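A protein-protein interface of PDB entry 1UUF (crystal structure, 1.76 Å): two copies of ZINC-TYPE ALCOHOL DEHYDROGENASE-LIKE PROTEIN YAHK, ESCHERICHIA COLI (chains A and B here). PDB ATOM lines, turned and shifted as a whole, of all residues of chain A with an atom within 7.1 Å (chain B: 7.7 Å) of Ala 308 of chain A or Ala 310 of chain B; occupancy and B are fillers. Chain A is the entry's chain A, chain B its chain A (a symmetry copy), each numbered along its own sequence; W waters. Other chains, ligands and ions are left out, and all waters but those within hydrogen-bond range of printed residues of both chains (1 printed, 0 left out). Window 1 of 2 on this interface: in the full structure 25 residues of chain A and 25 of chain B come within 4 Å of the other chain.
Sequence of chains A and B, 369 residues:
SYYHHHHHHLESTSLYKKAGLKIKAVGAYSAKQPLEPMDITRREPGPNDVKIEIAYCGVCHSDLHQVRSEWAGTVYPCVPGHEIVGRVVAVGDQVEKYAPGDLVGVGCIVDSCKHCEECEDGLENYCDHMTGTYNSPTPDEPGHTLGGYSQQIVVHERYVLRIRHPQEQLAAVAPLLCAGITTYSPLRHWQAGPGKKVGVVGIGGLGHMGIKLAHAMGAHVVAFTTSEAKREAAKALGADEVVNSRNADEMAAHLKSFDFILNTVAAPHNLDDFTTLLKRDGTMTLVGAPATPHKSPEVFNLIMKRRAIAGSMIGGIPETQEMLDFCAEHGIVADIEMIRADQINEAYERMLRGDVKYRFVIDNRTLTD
N of Gly 311 of chain B sits at hydrogen-bond distance from O of Arg 307 of chain A, at 3.2 Å. The backbone carbonyl oxygen (O) of Ile 309 of chain B is in hydrogen-bond range of the backbone NH (N) of Ile 309 of chain A (2.9 Å).
The backbone carbonyl oxygen (O) of Thr 275 of chain A is in hydrogen-bond range of the guanidinium group (NE) of Arg 307 of chain A (3.1 Å). N of Met 284 of chain A is in hydrogen-bond range of O of Ala 308 of chain A (3.0 Å). The backbone carbonyl oxygen (O) of Leu 302 of chain A lies within hydrogen-bond range of the backbone NH (N) of Arg 307 of chain A (2.9 Å). N of Met 284 of chain B sits at hydrogen-bond distance from O of Ala 308 of chain B, at 3.0 Å. The backbone carbonyl oxygen (O) of Met 284 of chain B sits at hydrogen-bond distance from the backbone NH (N) of Ala 310 of chain B, 2.9 Å away. The backbone carbonyl oxygen (O) of Leu 302 of chain B lies within hydrogen-bond range of the backbone NH (N) of Arg 307 of chain B (3.0 Å).
Among the printed residues, merely in contact across the chains: Arg 306 of chain A with Gly 311 of chain B, Ile 309 of chain A with Ala 308 of chain B, Ala 308 of chain A with Ile 309 of chain B, Ala 310 of chain A with Arg 307 of chain B, Arg 307 of chain A with Ala 310 of chain B, Ile 303 of chain A with Ser 312 of chain B, Ile 303 of chain A with Leu 286 of chain B, Val 299 of chain A with Leu 286 of chain B, Arg 306 of chain A with His 189 of chain B, Leu 302 of chain A with Gly 311 of chain B, Ala 310 of chain A with Ala 308 of chain B, Ala 308 of chain A with Ala 310 of chain B, Asp 281 of chain A with His 189 of chain B and Ile 303 of chain A with Gly 311 of chain B.
Ala 308 of chain A touches just these residues of chain B: Ile 309 and Ala 310. Met 284 of chain B touches none of the printed residues of chain A. Of the printed residues of chain A, Ala 308 of chain B touches Ile 309 and Ala 310. Ala 310 of chain B touches just these residues of chain A: Arg 307 (3.3 Å) and Ala 308 (3.7 Å). Of the printed residues of chain A, Gly 311 of chain B touches Leu 302 (3.7 Å), Ile 303 (3.8 Å), Arg 306 (3.2 Å) and Arg 307 (3.2 Å). Printed residues of chain A within 4 Å of Ser 312 of chain B: Ile 303. The nearest residue of chain A that does not touch Ala 310 of chain B is Leu 302 of chain A (4.3 Å).
Of the 19 printed residues of chain A, 9 touch a printed residue of chain B. Of the 17 printed residues of chain B, 8 touch a printed residue of chain A. Printed residues of chain B that touch a printed residue of chain A: His 189, Leu 286, Arg 307, Ala 308, Ile 309, Ala 310, Gly 311 and Ser 312. Among the printed residues, 16 pairs touch across the chains.
Arg 307 of chain A touches Ala 310 of chain B, and with the chains exchanged Ala 310 of chain A touches Arg 307 of chain B. Ala 308 of chain A touches Ile 309 of chain B, and with the chains exchanged Ile 309 of chain A touches Ala 308 of chain B. Ala 308 of chain A touches Ala 310 of chain B, and with the chains exchanged Ala 310 of chain A touches Ala 308 of chain B. Ile 309 of chain B touches its own counterpart, Ile 309 of chain A. 9 positions are printed for both chains.
Water W1 lies within hydrogen-bond range of OG of Ser 312 of chain B and NH1 of Arg 306 of chain A.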
ATOM      1  N   TRP A 190      23.327 -17.644  -9.444  1.00  0.00           N
ATOM      2  CA  TRP A 190      22.197 -16.726  -9.482  1.00  0.00           C
ATOM      3  C   TRP A 190      22.161 -15.823  -8.251  1.00  0.00           C
ATOM      4  O   TRP A 190      21.127 -15.271  -7.874  1.00  0.00           O
ATOM      5  CB  TRP A 190      20.893 -17.501  -9.690  1.00  0.00           C
ATOM      6  CG  TRP A 190      20.671 -17.803 -11.159  1.00  0.00           C
ATOM      7  CD1 TRP A 190      20.142 -16.958 -12.100  1.00  0.00           C
ATOM      8  CD2 TRP A 190      21.052 -18.995 -11.863  1.00  0.00           C
ATOM      9  NE1 TRP A 190      20.173 -17.553 -13.345  1.00  0.00           N
ATOM     10  CE2 TRP A 190      20.726 -18.802 -13.226  1.00  0.00           C
ATOM     11  CE3 TRP A 190      21.639 -20.208 -11.475  1.00  0.00           C
ATOM     12  CZ2 TRP A 190      20.965 -19.779 -14.202  1.00  0.00           C
ATOM     13  CZ3 TRP A 190      21.878 -21.178 -12.445  1.00  0.00           C
ATOM     14  CH2 TRP A 190      21.540 -20.956 -13.793  1.00  0.00           C
ATOM     15  N   THR A 275       6.811 -20.822 -12.217  1.00  0.00           N
ATOM     16  CA  THR A 275       7.250 -19.706 -13.045  1.00  0.00           C
ATOM     17  C   THR A 275       6.525 -18.425 -12.637  1.00  0.00           C
ATOM     18  O   THR A 275       7.122 -17.349 -12.599  1.00  0.00           O
ATOM     19  CB  THR A 275       7.001 -20.000 -14.537  1.00  0.00           C
ATOM     20  OG1 THR A 275       7.789 -21.132 -14.928  1.00  0.00           O
ATOM     21  CG2 THR A 275       7.393 -18.803 -15.393  1.00  0.00           C
ATOM     22  N   LEU A 278       8.030 -16.262  -9.817  1.00  0.00           N
ATOM     23  CA  LEU A 278       9.260 -15.510 -10.061  1.00  0.00           C
ATOM     24  C   LEU A 278       9.034 -14.025 -10.313  1.00  0.00           C
ATOM     25  O   LEU A 278       8.077 -13.643 -10.978  1.00  0.00           O
ATOM     26  CB  LEU A 278       9.991 -16.080 -11.276  1.00  0.00           C
ATOM     27  CG  LEU A 278      10.530 -17.505 -11.208  1.00  0.00           C
ATOM     28  CD1 LEU A 278      11.012 -17.917 -12.597  1.00  0.00           C
ATOM     29  CD2 LEU A 278      11.662 -17.578 -10.195  1.00  0.00           C
ATOM     30  N   LYS A 279       9.932 -13.194  -9.791  1.00  0.00           N
ATOM     31  CA  LYS A 279       9.852 -11.753 -10.009  1.00  0.00           C
ATOM     32  C   LYS A 279      10.300 -11.511 -11.442  1.00  0.00           C
ATOM     33  O   LYS A 279      10.766 -12.429 -12.118  1.00  0.00           O
ATOM     34  CB  LYS A 279      10.816 -11.011  -9.085  1.00  0.00           C
ATOM     35  CG  LYS A 279      10.489 -11.105  -7.608  1.00  0.00           C
ATOM     36  CD  LYS A 279      11.662 -10.629  -6.764  1.00  0.00           C
ATOM     37  CE  LYS A 279      12.047  -9.190  -7.083  1.00  0.00           C
ATOM     38  NZ  LYS A 279      13.179  -8.739  -6.225  1.00  0.00           N
ATOM     39  N   ASP A 281      12.554 -10.758 -14.390  1.00  0.00           N
ATOM     40  CA  ASP A 281      13.956 -11.112 -14.590  1.00  0.00           C
ATOM     41  C   ASP A 281      14.413 -12.245 -13.672  1.00  0.00           C
ATOM     42  O   ASP A 281      15.611 -12.497 -13.537  1.00  0.00           O
ATOM     43  CB  ASP A 281      14.869  -9.895 -14.396  1.00  0.00           C
ATOM     44  CG  ASP A 281      15.018  -9.070 -15.668  1.00  0.00           C
ATOM     45  OD1 ASP A 281      15.034  -9.670 -16.765  1.00  0.00           O
ATOM     46  OD2 ASP A 281      15.139  -7.829 -15.571  1.00  0.00           O
ATOM     47  N   GLY A 282      13.451 -12.928 -13.057  1.00  0.00           N
ATOM     48  CA  GLY A 282      13.770 -14.036 -12.172  1.00  0.00           C
ATOM     49  C   GLY A 282      14.024 -15.317 -12.945  1.00  0.00           C
ATOM     50  O   GLY A 282      13.605 -15.452 -14.091  1.00  0.00           O
ATOM     51  N   THR A 283      14.695 -16.273 -12.311  1.00  0.00           N
ATOM     52  CA  THR A 283      15.004 -17.532 -12.971  1.00  0.00           C
ATOM     53  C   THR A 283      14.731 -18.731 -12.081  1.00  0.00           C
ATOM     54  O   THR A 283      14.913 -18.658 -10.870  1.00  0.00           O
ATOM     55  CB  THR A 283      16.499 -17.596 -13.353  1.00  0.00           C
ATOM     56  OG1 THR A 283      16.801 -16.572 -14.305  1.00  0.00           O
ATOM     57  CG2 THR A 283      16.853 -18.965 -13.939  1.00  0.00           C
ATOM     58  N   MET A 284      14.269 -19.822 -12.685  1.00  0.00           N
ATOM     59  CA  MET A 284      14.083 -21.065 -11.940  1.00  0.00           C
ATOM     60  C   MET A 284      15.045 -22.016 -12.620  1.00  0.00           C
ATOM     61  O   MET A 284      14.974 -22.215 -13.834  1.00  0.00           O
ATOM     62  CB  MET A 284      12.666 -21.631 -12.039  1.00  0.00           C
ATOM     63  CG  MET A 284      12.598 -23.064 -11.484  1.00  0.00           C
ATOM     64  SD  MET A 284      10.932 -23.684 -11.193  1.00  0.00           S
ATOM     65  CE  MET A 284      10.263 -23.606 -12.855  1.00  0.00           C
ATOM     66  N   THR A 285      15.961 -22.583 -11.848  1.00  0.00           N
ATOM     67  CA  THR A 285      16.943 -23.500 -12.408  1.00  0.00           C
ATOM     68  C   THR A 285      16.674 -24.910 -11.927  1.00  0.00           C
ATOM     69  O   THR A 285      16.470 -25.136 -10.736  1.00  0.00           O
ATOM     70  CB  THR A 285      18.364 -23.084 -12.001  1.00  0.00           C
ATOM     71  OG1 THR A 285      18.643 -21.793 -12.553  1.00  0.00           O
ATOM     72  CG2 THR A 285      19.400 -24.087 -12.512  1.00  0.00           C
ATOM     73  N   VAL A 299       4.790 -20.459 -22.178  1.00  0.00           N
ATOM     74  CA  VAL A 299       5.655 -19.391 -22.668  1.00  0.00           C
ATOM     75  C   VAL A 299       5.151 -18.020 -22.235  1.00  0.00           C
ATOM     76  O   VAL A 299       5.941 -17.117 -21.970  1.00  0.00           O
ATOM     77  CB  VAL A 299       5.761 -19.422 -24.208  1.00  0.00           C
ATOM     78  CG1 VAL A 299       6.651 -18.287 -24.692  1.00  0.00           C
ATOM     79  CG2 VAL A 299       6.323 -20.762 -24.658  1.00  0.00           C
ATOM     80  N   ASN A 301       3.974 -16.960 -19.485  1.00  0.00           N
ATOM     81  CA  ASN A 301       4.519 -16.556 -18.197  1.00  0.00           C
ATOM     82  C   ASN A 301       5.984 -16.142 -18.253  1.00  0.00           C
ATOM     83  O   ASN A 301       6.438 -15.354 -17.425  1.00  0.00           O
ATOM     84  CB  ASN A 301       4.315 -17.669 -17.166  1.00  0.00           C
ATOM     85  CG  ASN A 301       2.847 -17.926 -16.883  1.00  0.00           C
ATOM     86  OD1 ASN A 301       2.083 -16.992 -16.633  1.00  0.00           O
ATOM     87  ND2 ASN A 301       2.445 -19.191 -16.917  1.00  0.00           N
ATOM     88  N   LEU A 302       6.727 -16.660 -19.227  1.00  0.00           N
ATOM     89  CA  LEU A 302       8.129 -16.279 -19.356  1.00  0.00           C
ATOM     90  C   LEU A 302       8.202 -14.903 -20.006  1.00  0.00           C
ATOM     91  O   LEU A 302       8.970 -14.040 -19.589  1.00  0.00           O
ATOM     92  CB  LEU A 302       8.898 -17.276 -20.230  1.00  0.00           C
ATOM     93  CG  LEU A 302       9.091 -18.704 -19.718  1.00  0.00           C
ATOM     94  CD1 LEU A 302       9.925 -19.477 -20.721  1.00  0.00           C
ATOM     95  CD2 LEU A 302       9.771 -18.684 -18.358  1.00  0.00           C
ATOM     96  N   ILE A 303       7.386 -14.706 -21.034  1.00  0.00           N
ATOM     97  CA  ILE A 303       7.362 -13.443 -21.764  1.00  0.00           C
ATOM     98  C   ILE A 303       6.892 -12.241 -20.953  1.00  0.00           C
ATOM     99  O   ILE A 303       7.526 -11.188 -20.972  1.00  0.00           O
ATOM    100  CB  ILE A 303       6.482 -13.573 -23.023  1.00  0.00           C
ATOM    101  CG1 ILE A 303       7.209 -14.436 -24.054  1.00  0.00           C
ATOM    102  CG2 ILE A 303       6.164 -12.200 -23.601  1.00  0.00           C
ATOM    103  CD1 ILE A 303       6.380 -14.761 -25.277  1.00  0.00           C
ATOM    104  N   LYS A 305       7.134 -11.366 -17.952  1.00  0.00           N
ATOM    105  CA  LYS A 305       8.024 -10.792 -16.946  1.00  0.00           C
ATOM    106  C   LYS A 305       9.499 -11.043 -17.216  1.00  0.00           C
ATOM    107  O   LYS A 305      10.326 -10.896 -16.316  1.00  0.00           O
ATOM    108  CB  LYS A 305       7.673 -11.344 -15.560  1.00  0.00           C
ATOM    109  CG  LYS A 305       6.315 -10.897 -15.032  1.00  0.00           C
ATOM    110  CD  LYS A 305       6.312  -9.413 -14.710  1.00  0.00           C
ATOM    111  CE  LYS A 305       5.002  -9.001 -14.056  1.00  0.00           C
ATOM    112  NZ  LYS A 305       4.964  -7.538 -13.797  1.00  0.00           N
ATOM    113  N   ARG A 306       9.822 -11.408 -18.451  1.00  0.00           N
ATOM    114  CA  ARG A 306      11.198 -11.699 -18.840  1.00  0.00           C
ATOM    115  C   ARG A 306      11.838 -12.665 -17.850  1.00  0.00           C
ATOM    116  O   ARG A 306      12.916 -12.412 -17.302  1.00  0.00           O
ATOM    117  CB  ARG A 306      12.028 -10.413 -18.930  1.00  0.00           C
ATOM    118  CG  ARG A 306      13.322 -10.615 -19.715  1.00  0.00           C
ATOM    119  CD  ARG A 306      13.880  -9.292 -20.224  1.00  0.00           C
ATOM    120  NE  ARG A 306      14.283  -8.415 -19.129  1.00  0.00           N
ATOM    121  CZ  ARG A 306      14.648  -7.148 -19.282  1.00  0.00           C
ATOM    122  NH1 ARG A 306      14.659  -6.597 -20.491  1.00  0.00           N
ATOM    123  NH2 ARG A 306      15.005  -6.430 -18.224  1.00  0.00           N
ATOM    124  N   ARG A 307      11.150 -13.776 -17.620  1.00  0.00           N
ATOM    125  CA  ARG A 307      11.631 -14.805 -16.708  1.00  0.00           C
ATOM    126  C   ARG A 307      12.347 -15.859 -17.527  1.00  0.00           C
ATOM    127  O   ARG A 307      12.243 -15.880 -18.752  1.00  0.00           O
ATOM    128  CB  ARG A 307      10.461 -15.458 -15.989  1.00  0.00           C
ATOM    129  CG  ARG A 307       9.724 -14.559 -15.026  1.00  0.00           C
ATOM    130  CD  ARG A 307       8.309 -15.069 -14.872  1.00  0.00           C
ATOM    131  NE  ARG A 307       7.592 -14.460 -13.760  1.00  0.00           N
ATOM    132  CZ  ARG A 307       6.270 -14.349 -13.712  1.00  0.00           C
ATOM    133  NH1 ARG A 307       5.531 -14.796 -14.719  1.00  0.00           N
ATOM    134  NH2 ARG A 307       5.687 -13.808 -12.652  1.00  0.00           N
ATOM    135  N   ALA A 308      13.070 -16.740 -16.847  1.00  0.00           N
ATOM    136  CA  ALA A 308      13.790 -17.790 -17.541  1.00  0.00           C
ATOM    137  C   ALA A 308      13.804 -19.093 -16.759  1.00  0.00           C
ATOM    138  O   ALA A 308      13.666 -19.104 -15.530  1.00  0.00           O
ATOM    139  CB  ALA A 308      15.225 -17.341 -17.803  1.00  0.00           C
ATOM    140  N   ILE A 309      13.950 -20.189 -17.494  1.00  0.00           N
ATOM    141  CA  ILE A 309      14.073 -21.509 -16.899  1.00  0.00           C
ATOM    142  C   ILE A 309      15.450 -21.955 -17.369  1.00  0.00           C
ATOM    143  O   ILE A 309      15.757 -21.888 -18.556  1.00  0.00           O
ATOM    144  CB  ILE A 309      13.006 -22.488 -17.425  1.00  0.00           C
ATOM    145  CG1 ILE A 309      11.608 -21.953 -17.109  1.00  0.00           C
ATOM    146  CG2 ILE A 309      13.211 -23.864 -16.796  1.00  0.00           C
ATOM    147  CD1 ILE A 309      11.368 -21.668 -15.644  1.00  0.00           C
ATOM    148  N   ALA A 310      16.286 -22.387 -16.437  1.00  0.00           N
ATOM    149  CA  ALA A 310      17.631 -22.811 -16.783  1.00  0.00           C
ATOM    150  C   ALA A 310      17.945 -24.154 -16.152  1.00  0.00           C
ATOM    151  O   ALA A 310      17.138 -24.720 -15.418  1.00  0.00           O
ATOM    152  CB  ALA A 310      18.640 -21.767 -16.311  1.00  0.00           C
ATOM    153  N   HIS B 189      19.468  -6.787 -24.298  1.00  0.00           N
ATOM    154  CA  HIS B 189      19.549  -7.417 -22.981  1.00  0.00           C
ATOM    155  C   HIS B 189      20.543  -8.569 -22.940  1.00  0.00           C
ATOM    156  O   HIS B 189      21.283  -8.721 -21.964  1.00  0.00           O
ATOM    157  CB  HIS B 189      18.176  -7.915 -22.528  1.00  0.00           C
ATOM    158  CG  HIS B 189      18.114  -8.241 -21.069  1.00  0.00           C
ATOM    159  ND1 HIS B 189      17.876  -9.514 -20.597  1.00  0.00           N
ATOM    160  CD2 HIS B 189      18.267  -7.457 -19.976  1.00  0.00           C
ATOM    161  CE1 HIS B 189      17.883  -9.499 -19.275  1.00  0.00           C
ATOM    162  NE2 HIS B 189      18.118  -8.263 -18.873  1.00  0.00           N
ATOM    163  N   TRP B 190      20.569  -9.381 -23.992  1.00  0.00           N
ATOM    164  CA  TRP B 190      21.498 -10.502 -24.032  1.00  0.00           C
ATOM    165  C   TRP B 190      22.778 -10.148 -24.785  1.00  0.00           C
ATOM    166  O   TRP B 190      23.505 -11.010 -25.280  1.00  0.00           O
ATOM    167  CB  TRP B 190      20.802 -11.746 -24.592  1.00  0.00           C
ATOM    168  CG  TRP B 190      20.017 -12.460 -23.509  1.00  0.00           C
ATOM    169  CD1 TRP B 190      20.512 -13.340 -22.581  1.00  0.00           C
ATOM    170  CD2 TRP B 190      18.627 -12.286 -23.192  1.00  0.00           C
ATOM    171  NE1 TRP B 190      19.514 -13.721 -21.707  1.00  0.00           N
ATOM    172  CE2 TRP B 190      18.350 -13.090 -22.061  1.00  0.00           C
ATOM    173  CE3 TRP B 190      17.589 -11.529 -23.753  1.00  0.00           C
ATOM    174  CZ2 TRP B 190      17.075 -13.158 -21.483  1.00  0.00           C
ATOM    175  CZ3 TRP B 190      16.323 -11.596 -23.177  1.00  0.00           C
ATOM    176  CH2 TRP B 190      16.079 -12.406 -22.054  1.00  0.00           C
ATOM    177  N   PHE B 260      23.429 -16.442 -28.309  1.00  0.00           N
ATOM    178  CA  PHE B 260      22.044 -16.074 -28.076  1.00  0.00           C
ATOM    179  C   PHE B 260      21.176 -16.409 -29.287  1.00  0.00           C
ATOM    180  O   PHE B 260      21.608 -16.272 -30.428  1.00  0.00           O
ATOM    181  CB  PHE B 260      21.988 -14.570 -27.792  1.00  0.00           C
ATOM    182  CG  PHE B 260      20.600 -14.025 -27.630  1.00  0.00           C
ATOM    183  CD1 PHE B 260      19.781 -14.463 -26.596  1.00  0.00           C
ATOM    184  CD2 PHE B 260      20.117 -13.057 -28.507  1.00  0.00           C
ATOM    185  CE1 PHE B 260      18.497 -13.944 -26.436  1.00  0.00           C
ATOM    186  CE2 PHE B 260      18.837 -12.532 -28.357  1.00  0.00           C
ATOM    187  CZ  PHE B 260      18.024 -12.978 -27.318  1.00  0.00           C
ATOM    188  N   ILE B 261      19.959 -16.869 -29.030  1.00  0.00           N
ATOM    189  CA  ILE B 261      19.033 -17.176 -30.105  1.00  0.00           C
ATOM    190  C   ILE B 261      17.713 -16.482 -29.817  1.00  0.00           C
ATOM    191  O   ILE B 261      17.115 -16.679 -28.763  1.00  0.00           O
ATOM    192  CB  ILE B 261      18.773 -18.691 -30.243  1.00  0.00           C
ATOM    193  CG1 ILE B 261      20.041 -19.390 -30.742  1.00  0.00           C
ATOM    194  CG2 ILE B 261      17.642 -18.934 -31.244  1.00  0.00           C
ATOM    195  CD1 ILE B 261      19.901 -20.888 -30.886  1.00  0.00           C
ATOM    196  N   ASN B 263      14.012 -16.326 -30.799  1.00  0.00           N
ATOM    197  CA  ASN B 263      12.985 -17.083 -31.512  1.00  0.00           C
ATOM    198  C   ASN B 263      11.715 -16.243 -31.630  1.00  0.00           C
ATOM    199  O   ASN B 263      11.064 -15.955 -30.628  1.00  0.00           O
ATOM    200  CB  ASN B 263      12.719 -18.399 -30.773  1.00  0.00           C
ATOM    201  CG  ASN B 263      11.933 -19.392 -31.610  1.00  0.00           C
ATOM    202  OD1 ASN B 263      12.166 -20.604 -31.544  1.00  0.00           O
ATOM    203  ND2 ASN B 263      10.995 -18.887 -32.392  1.00  0.00           N
ATOM    204  N   THR B 283      21.496 -18.532 -24.083  1.00  0.00           N
ATOM    205  CA  THR B 283      20.065 -18.406 -23.855  1.00  0.00           C
ATOM    206  C   THR B 283      19.284 -18.271 -25.149  1.00  0.00           C
ATOM    207  O   THR B 283      19.767 -17.672 -26.105  1.00  0.00           O
ATOM    208  CB  THR B 283      19.754 -17.146 -23.018  1.00  0.00           C
ATOM    209  OG1 THR B 283      20.348 -17.265 -21.722  1.00  0.00           O
ATOM    210  CG2 THR B 283      18.243 -16.945 -22.876  1.00  0.00           C
ATOM    211  N   MET B 284      18.088 -18.853 -25.181  1.00  0.00           N
ATOM    212  CA  MET B 284      17.209 -18.687 -26.336  1.00  0.00           C
ATOM    213  C   MET B 284      16.006 -17.978 -25.748  1.00  0.00           C
ATOM    214  O   MET B 284      15.396 -18.466 -24.795  1.00  0.00           O
ATOM    215  CB  MET B 284      16.755 -20.010 -26.955  1.00  0.00           C
ATOM    216  CG  MET B 284      15.621 -19.789 -27.971  1.00  0.00           C
ATOM    217  SD  MET B 284      15.275 -21.201 -29.034  1.00  0.00           S
ATOM    218  CE  MET B 284      14.810 -22.425 -27.807  1.00  0.00           C
ATOM    219  N   THR B 285      15.681 -16.814 -26.293  1.00  0.00           N
ATOM    220  CA  THR B 285      14.553 -16.045 -25.790  1.00  0.00           C
ATOM    221  C   THR B 285      13.430 -16.041 -26.805  1.00  0.00           C
ATOM    222  O   THR B 285      13.657 -15.791 -27.986  1.00  0.00           O
ATOM    223  CB  THR B 285      14.975 -14.600 -25.488  1.00  0.00           C
ATOM    224  OG1 THR B 285      15.961 -14.614 -24.451  1.00  0.00           O
ATOM    225  CG2 THR B 285      13.779 -13.759 -25.039  1.00  0.00           C
ATOM    226  N   LEU B 286      12.220 -16.323 -26.332  1.00  0.00           N
ATOM    227  CA  LEU B 286      11.046 -16.366 -27.191  1.00  0.00           C
ATOM    228  C   LEU B 286      10.300 -15.031 -27.124  1.00  0.00           C
ATOM    229  O   LEU B 286      10.117 -14.476 -26.042  1.00  0.00           O
ATOM    230  CB  LEU B 286      10.110 -17.488 -26.728  1.00  0.00           C
ATOM    231  CG  LEU B 286      10.762 -18.820 -26.344  1.00  0.00           C
ATOM    232  CD1 LEU B 286       9.699 -19.777 -25.826  1.00  0.00           C
ATOM    233  CD2 LEU B 286      11.482 -19.407 -27.536  1.00  0.00           C
ATOM    234  N   VAL B 287       9.879 -14.515 -28.276  1.00  0.00           N
ATOM    235  CA  VAL B 287       9.130 -13.259 -28.305  1.00  0.00           C
ATOM    236  C   VAL B 287       7.868 -13.353 -29.155  1.00  0.00           C
ATOM    237  O   VAL B 287       7.058 -12.424 -29.176  1.00  0.00           O
ATOM    238  CB  VAL B 287       9.990 -12.076 -28.826  1.00  0.00           C
ATOM    239  CG1 VAL B 287      11.140 -11.821 -27.880  1.00  0.00           C
ATOM    240  CG2 VAL B 287      10.502 -12.375 -30.230  1.00  0.00           C
ATOM    241  N   LEU B 302      19.298 -28.409 -21.070  1.00  0.00           N
ATOM    242  CA  LEU B 302      19.500 -27.171 -20.325  1.00  0.00           C
ATOM    243  C   LEU B 302      20.546 -27.417 -19.245  1.00  0.00           C
ATOM    244  O   LEU B 302      21.438 -26.603 -19.025  1.00  0.00           O
ATOM    245  CB  LEU B 302      18.201 -26.709 -19.655  1.00  0.00           C
ATOM    246  CG  LEU B 302      17.037 -26.262 -20.540  1.00  0.00           C
ATOM    247  CD1 LEU B 302      15.897 -25.798 -19.654  1.00  0.00           C
ATOM    248  CD2 LEU B 302      17.486 -25.142 -21.467  1.00  0.00           C
ATOM    249  N   ARG B 307      22.215 -23.882 -19.859  1.00  0.00           N
ATOM    250  CA  ARG B 307      21.541 -23.048 -20.845  1.00  0.00           C
ATOM    251  C   ARG B 307      20.214 -22.611 -20.262  1.00  0.00           C
ATOM    252  O   ARG B 307      19.768 -23.144 -19.247  1.00  0.00           O
ATOM    253  CB  ARG B 307      21.278 -23.842 -22.114  1.00  0.00           C
ATOM    254  CG  ARG B 307      22.514 -24.237 -22.886  1.00  0.00           C
ATOM    255  CD  ARG B 307      22.202 -25.471 -23.703  1.00  0.00           C
ATOM    256  NE  ARG B 307      23.219 -25.777 -24.700  1.00  0.00           N
ATOM    257  CZ  ARG B 307      23.442 -26.998 -25.170  1.00  0.00           C
ATOM    258  NH1 ARG B 307      22.725 -28.021 -24.722  1.00  0.00           N
ATOM    259  NH2 ARG B 307      24.366 -27.194 -26.099  1.00  0.00           N
ATOM    260  N   ALA B 308      19.578 -21.642 -20.908  1.00  0.00           N
ATOM    261  CA  ALA B 308      18.298 -21.157 -20.429  1.00  0.00           C
ATOM    262  C   ALA B 308      17.360 -20.788 -21.565  1.00  0.00           C
ATOM    263  O   ALA B 308      17.796 -20.476 -22.680  1.00  0.00           O
ATOM    264  CB  ALA B 308      18.513 -19.940 -19.533  1.00  0.00           C
ATOM    265  N   ILE B 309      16.067 -20.849 -21.270  1.00  0.00           N
ATOM    266  CA  ILE B 309      15.038 -20.444 -22.213  1.00  0.00           C
ATOM    267  C   ILE B 309      14.350 -19.303 -21.479  1.00  0.00           C
ATOM    268  O   ILE B 309      13.968 -19.446 -20.321  1.00  0.00           O
ATOM    269  CB  ILE B 309      14.021 -21.569 -22.488  1.00  0.00           C
ATOM    270  CG1 ILE B 309      14.740 -22.791 -23.065  1.00  0.00           C
ATOM    271  CG2 ILE B 309      12.946 -21.072 -23.451  1.00  0.00           C
ATOM    272  CD1 ILE B 309      15.543 -22.506 -24.313  1.00  0.00           C
ATOM    273  N   ALA B 310      14.213 -18.165 -22.143  1.00  0.00           N
ATOM    274  CA  ALA B 310      13.592 -17.010 -21.519  1.00  0.00           C
ATOM    275  C   ALA B 310      12.539 -16.412 -22.433  1.00  0.00           C
ATOM    276  O   ALA B 310      12.334 -16.869 -23.556  1.00  0.00           O
ATOM    277  CB  ALA B 310      14.654 -15.962 -21.196  1.00  0.00           C
ATOM    278  N   GLY B 311      11.858 -15.396 -21.924  1.00  0.00           N
ATOM    279  CA  GLY B 311      10.847 -14.719 -22.708  1.00  0.00           C
ATOM    280  C   GLY B 311      11.091 -13.231 -22.590  1.00  0.00           C
ATOM    281  O   GLY B 311      11.845 -12.788 -21.725  1.00  0.00           O
ATOM    282  N   SER B 312      10.468 -12.454 -23.464  1.00  0.00           N
ATOM    283  CA  SER B 312      10.620 -11.008 -23.425  1.00  0.00           C
ATOM    284  C   SER B 312       9.480 -10.388 -24.215  1.00  0.00           C
ATOM    285  O   SER B 312       9.006 -10.982 -25.179  1.00  0.00           O
ATOM    286  CB  SER B 312      11.961 -10.599 -24.049  1.00  0.00           C
ATOM    287  OG  SER B 312      12.123  -9.187 -24.057  1.00  0.00           O
HETATM  288  O   HOH W   1      14.482  -7.705 -23.226  1.00  0.00           O
